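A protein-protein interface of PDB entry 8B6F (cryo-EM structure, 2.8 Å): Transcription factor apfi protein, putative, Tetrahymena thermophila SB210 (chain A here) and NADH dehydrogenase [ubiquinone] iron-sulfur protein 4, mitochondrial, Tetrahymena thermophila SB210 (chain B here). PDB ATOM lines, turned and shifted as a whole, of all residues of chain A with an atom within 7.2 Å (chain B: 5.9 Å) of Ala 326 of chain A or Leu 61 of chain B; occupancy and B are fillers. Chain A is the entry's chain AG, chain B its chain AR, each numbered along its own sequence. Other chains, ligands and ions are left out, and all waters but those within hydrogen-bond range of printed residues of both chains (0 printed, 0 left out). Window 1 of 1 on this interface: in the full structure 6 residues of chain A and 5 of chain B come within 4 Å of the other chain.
OE2 of Glu 325 of chain A touches OD2 of Asp 62 of chain B, 3.5 Å away. Ile 328 of chain A touches Arg 79 of chain B (CD1 to NH2, 3.1 Å).
The side-chain sulfur of Cys 65 of chain B sits at hydrogen-bond distance from the backbone carbonyl oxygen of Asp 62 of chain B (3.3 Å).
The side-chain carboxylate of Glu 325 of chain A sits close to the backbone carbonyl oxygen of Leu 61 of chain B (2.6 Å). O of Val 324 of chain A lies close to OD1 of Asp 62 of chain B (2.5 Å). The backbone carbonyl oxygen (O) of Val 324 of chain A lies within hydrogen-bond range of the backbone NH (N) of Ser 63 of chain B (3.0 Å). The backbone NH of Ala 326 of chain A sits at hydrogen-bond distance from the backbone carbonyl oxygen of Leu 61 of chain B, at 3.4 Å.
Of the 6 printed residues of chain A, 4 touch a printed residue of chain B. Hydrophobic or aromatic side chains of chain A within 4 Å of the printed part of chain B: Ile 328. Along chain A the printed residues that touch a printed residue of chain B span positions 324 to 328. Of the 10 printed residues of chain B, 4 touch a printed residue of chain A. Printed residues of chain B that touch a printed residue of chain A: Leu 61, Asp 62, Ser 63 and Arg 79. Among the printed residues, 6 pairs touch across the chains.
Of chain B, only Leu 61 comes within 4 Å of Ala 326 of chain A. Of chain A, only Glu 325 and Ala 326 come within 4 Å of Leu 61 of chain B. Of the printed residues of chain B, Val 324 of chain A touches Asp 62 (2.5 Å) and Ser 63 (3.0 Å). Of the printed residues of chain B, Glu 325 of chain A touches Leu 61 (2.6 Å) and Asp 62 (3.5 Å). Printed residues of chain A within 4 Å of Asp 62 of chain B: Val 324 (2.5 Å) and Glu 325 (3.5 Å). Printed residues of chain A within 4 Å of Arg 79 of chain B: Ile 328 (3.1 Å). The nearest residue of chain B that does not touch Ala 326 of chain A is Asp 62 of chain B (4.2 Å). The nearest printed residue of chain A that does not touch Arg 79 of chain B is Ala 326 of chain A (4.4 Å).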
ATOM      1  N   VAL A 324       0.326 -26.642  15.646  1.00  0.00           N
ATOM      2  CA  VAL A 324      -0.478 -25.483  16.007  1.00  0.00           C
ATOM      3  C   VAL A 324       0.195 -24.217  15.495  1.00  0.00           C
ATOM      4  O   VAL A 324       1.399 -24.181  15.237  1.00  0.00           O
ATOM      5  CB  VAL A 324      -0.703 -25.386  17.532  1.00  0.00           C
ATOM      6  CG1 VAL A 324      -1.370 -26.646  18.055  1.00  0.00           C
ATOM      7  CG2 VAL A 324       0.615 -25.133  18.258  1.00  0.00           C
ATOM      8  N   GLU A 325      -0.609 -23.165  15.359  1.00  0.00           N
ATOM      9  CA  GLU A 325      -0.101 -21.878  14.910  1.00  0.00           C
ATOM     10  C   GLU A 325       0.687 -21.191  16.020  1.00  0.00           C
ATOM     11  O   GLU A 325       0.415 -21.368  17.210  1.00  0.00           O
ATOM     12  CB  GLU A 325      -1.253 -20.980  14.461  1.00  0.00           C
ATOM     13  CG  GLU A 325      -2.057 -21.542  13.303  1.00  0.00           C
ATOM     14  CD  GLU A 325      -1.259 -21.606  12.016  1.00  0.00           C
ATOM     15  OE1 GLU A 325      -0.336 -20.784  11.849  1.00  0.00           O
ATOM     16  OE2 GLU A 325      -1.554 -22.478  11.172  1.00  0.00           O
ATOM     17  N   ALA A 326       1.674 -20.395  15.619  1.00  0.00           N
ATOM     18  CA  ALA A 326       2.520 -19.683  16.568  1.00  0.00           C
ATOM     19  C   ALA A 326       1.769 -18.475  17.115  1.00  0.00           C
ATOM     20  O   ALA A 326       1.332 -17.610  16.350  1.00  0.00           O
ATOM     21  CB  ALA A 326       3.823 -19.251  15.900  1.00  0.00           C
ATOM     22  N   THR A 327       1.625 -18.414  18.436  1.00  0.00           N
ATOM     23  CA  THR A 327       0.897 -17.318  19.060  1.00  0.00           C
ATOM     24  C   THR A 327       1.667 -16.012  18.915  1.00  0.00           C
ATOM     25  O   THR A 327       2.889 -15.969  19.078  1.00  0.00           O
ATOM     26  CB  THR A 327       0.655 -17.616  20.541  1.00  0.00           C
ATOM     27  OG1 THR A 327      -0.027 -18.869  20.677  1.00  0.00           O
ATOM     28  CG2 THR A 327      -0.187 -16.521  21.180  1.00  0.00           C
ATOM     29  N   ILE A 328       0.942 -14.941  18.603  1.00  0.00           N
ATOM     30  CA  ILE A 328       1.506 -13.603  18.489  1.00  0.00           C
ATOM     31  C   ILE A 328       0.775 -12.700  19.471  1.00  0.00           C
ATOM     32  O   ILE A 328      -0.459 -12.615  19.442  1.00  0.00           O
ATOM     33  CB  ILE A 328       1.393 -13.056  17.053  1.00  0.00           C
ATOM     34  CG1 ILE A 328       2.061 -14.009  16.057  1.00  0.00           C
ATOM     35  CG2 ILE A 328       2.009 -11.665  16.960  1.00  0.00           C
ATOM     36  CD1 ILE A 328       3.547 -14.212  16.281  1.00  0.00           C
ATOM     37  N   ILE A 329       1.532 -12.033  20.337  1.00  0.00           N
ATOM     38  CA  ILE A 329       0.982 -11.113  21.326  1.00  0.00           C
ATOM     39  C   ILE A 329       1.058  -9.707  20.748  1.00  0.00           C
ATOM     40  O   ILE A 329       2.141  -9.241  20.370  1.00  0.00           O
ATOM     41  CB  ILE A 329       1.735 -11.207  22.662  1.00  0.00           C
ATOM     42  CG1 ILE A 329       1.685 -12.636  23.215  1.00  0.00           C
ATOM     43  CG2 ILE A 329       1.162 -10.219  23.672  1.00  0.00           C
ATOM     44  CD1 ILE A 329       0.293 -13.145  23.529  1.00  0.00           C
ATOM     45  N   LYS B  25      -7.505 -16.566   7.773  1.00  0.00           N
ATOM     46  CA  LYS B  25      -7.607 -16.336   9.208  1.00  0.00           C
ATOM     47  C   LYS B  25      -7.993 -14.903   9.539  1.00  0.00           C
ATOM     48  O   LYS B  25      -8.940 -14.683  10.303  1.00  0.00           O
ATOM     49  CB  LYS B  25      -6.278 -16.693   9.890  1.00  0.00           C
ATOM     50  CG  LYS B  25      -6.309 -16.565  11.409  1.00  0.00           C
ATOM     51  CD  LYS B  25      -5.017 -17.061  12.046  1.00  0.00           C
ATOM     52  CE  LYS B  25      -3.834 -16.175  11.688  1.00  0.00           C
ATOM     53  NZ  LYS B  25      -2.579 -16.630  12.354  1.00  0.00           N
ATOM     54  N   PRO B  59       4.622 -16.366   4.620  1.00  0.00           N
ATOM     55  CA  PRO B  59       5.308 -17.004   5.747  1.00  0.00           C
ATOM     56  C   PRO B  59       4.372 -17.943   6.489  1.00  0.00           C
ATOM     57  O   PRO B  59       3.196 -17.639   6.696  1.00  0.00           O
ATOM     58  CB  PRO B  59       5.735 -15.820   6.621  1.00  0.00           C
ATOM     59  CG  PRO B  59       4.789 -14.733   6.267  1.00  0.00           C
ATOM     60  CD  PRO B  59       4.487 -14.913   4.811  1.00  0.00           C
ATOM     61  N   GLN B  60       4.904 -19.091   6.892  1.00  0.00           N
ATOM     62  CA  GLN B  60       4.131 -20.118   7.585  1.00  0.00           C
ATOM     63  C   GLN B  60       4.518 -20.081   9.060  1.00  0.00           C
ATOM     64  O   GLN B  60       5.391 -20.823   9.508  1.00  0.00           O
ATOM     65  CB  GLN B  60       4.383 -21.490   6.972  1.00  0.00           C
ATOM     66  CG  GLN B  60       3.466 -22.574   7.505  1.00  0.00           C
ATOM     67  CD  GLN B  60       3.646 -23.887   6.776  1.00  0.00           C
ATOM     68  OE1 GLN B  60       4.599 -24.065   6.018  1.00  0.00           O
ATOM     69  NE2 GLN B  60       2.725 -24.819   6.998  1.00  0.00           N
ATOM     70  N   LEU B  61       3.853 -19.209   9.815  1.00  0.00           N
ATOM     71  CA  LEU B  61       4.066 -19.111  11.256  1.00  0.00           C
ATOM     72  C   LEU B  61       3.296 -20.247  11.910  1.00  0.00           C
ATOM     73  O   LEU B  61       2.135 -20.107  12.293  1.00  0.00           O
ATOM     74  CB  LEU B  61       3.626 -17.750  11.782  1.00  0.00           C
ATOM     75  CG  LEU B  61       4.374 -16.506  11.282  1.00  0.00           C
ATOM     76  CD1 LEU B  61       5.882 -16.687  11.391  1.00  0.00           C
ATOM     77  CD2 LEU B  61       3.984 -16.138   9.857  1.00  0.00           C
ATOM     78  N   ASP B  62       3.960 -21.391  12.042  1.00  0.00           N
ATOM     79  CA  ASP B  62       3.332 -22.614  12.516  1.00  0.00           C
ATOM     80  C   ASP B  62       4.318 -23.305  13.450  1.00  0.00           C
ATOM     81  O   ASP B  62       5.320 -22.718  13.868  1.00  0.00           O
ATOM     82  CB  ASP B  62       2.934 -23.492  11.323  1.00  0.00           C
ATOM     83  CG  ASP B  62       1.832 -24.471  11.658  1.00  0.00           C
ATOM     84  OD1 ASP B  62       1.738 -24.876  12.833  1.00  0.00           O
ATOM     85  OD2 ASP B  62       1.061 -24.837  10.745  1.00  0.00           O
ATOM     86  N   SER B  63       4.037 -24.564  13.790  1.00  0.00           N
ATOM     87  CA  SER B  63       4.993 -25.333  14.572  1.00  0.00           C
ATOM     88  C   SER B  63       6.250 -25.664  13.781  1.00  0.00           C
ATOM     89  O   SER B  63       7.251 -26.068  14.381  1.00  0.00           O
ATOM     90  CB  SER B  63       4.350 -26.625  15.077  1.00  0.00           C
ATOM     91  OG  SER B  63       3.952 -27.452  13.998  1.00  0.00           O
ATOM     92  N   CYS B  65       8.178 -23.585  12.083  1.00  0.00           N
ATOM     93  CA  CYS B  65       9.179 -22.529  12.177  1.00  0.00           C
ATOM     94  C   CYS B  65       9.757 -22.397  13.579  1.00  0.00           C
ATOM     95  O   CYS B  65      10.203 -21.310  13.966  1.00  0.00           O
ATOM     96  CB  CYS B  65       8.579 -21.196  11.722  1.00  0.00           C
ATOM     97  SG  CYS B  65       7.514 -20.397  12.939  1.00  0.00           S
ATOM     98  N   ARG B  79      11.414 -12.482  11.769  1.00  0.00           N
ATOM     99  CA  ARG B  79      10.553 -13.612  11.456  1.00  0.00           C
ATOM    100  C   ARG B  79       9.319 -13.141  10.699  1.00  0.00           C
ATOM    101  O   ARG B  79       8.791 -12.054  10.952  1.00  0.00           O
ATOM    102  CB  ARG B  79      10.139 -14.343  12.732  1.00  0.00           C
ATOM    103  CG  ARG B  79       9.431 -15.662  12.464  1.00  0.00           C
ATOM    104  CD  ARG B  79       9.001 -16.343  13.750  1.00  0.00           C
ATOM    105  NE  ARG B  79       7.995 -15.568  14.467  1.00  0.00           N
ATOM    106  CZ  ARG B  79       7.383 -15.976  15.569  1.00  0.00           C
ATOM    107  NH1 ARG B  79       7.644 -17.153  16.112  1.00  0.00           N
ATOM    108  NH2 ARG B  79       6.484 -15.181  16.143  1.00  0.00           N
ATOM    109  N   GLY B  80       8.859 -13.968   9.764  1.00  0.00           N
ATOM    110  CA  GLY B  80       7.726 -13.624   8.936  1.00  0.00           C
ATOM    111  C   GLY B  80       8.050 -12.751   7.745  1.00  0.00           C
ATOM    112  O   GLY B  80       7.141 -12.428   6.971  1.00  0.00           O
ATOM    113  N   GLY B 150      10.590 -19.877   9.182  1.00  0.00           N
ATOM    114  CA  GLY B 150       9.342 -19.143   9.183  1.00  0.00           C
ATOM    115  C   GLY B 150       9.310 -17.934   8.277  1.00  0.00           C
ATOM    116  O   GLY B 150       8.491 -17.037   8.492  1.00  0.00           O
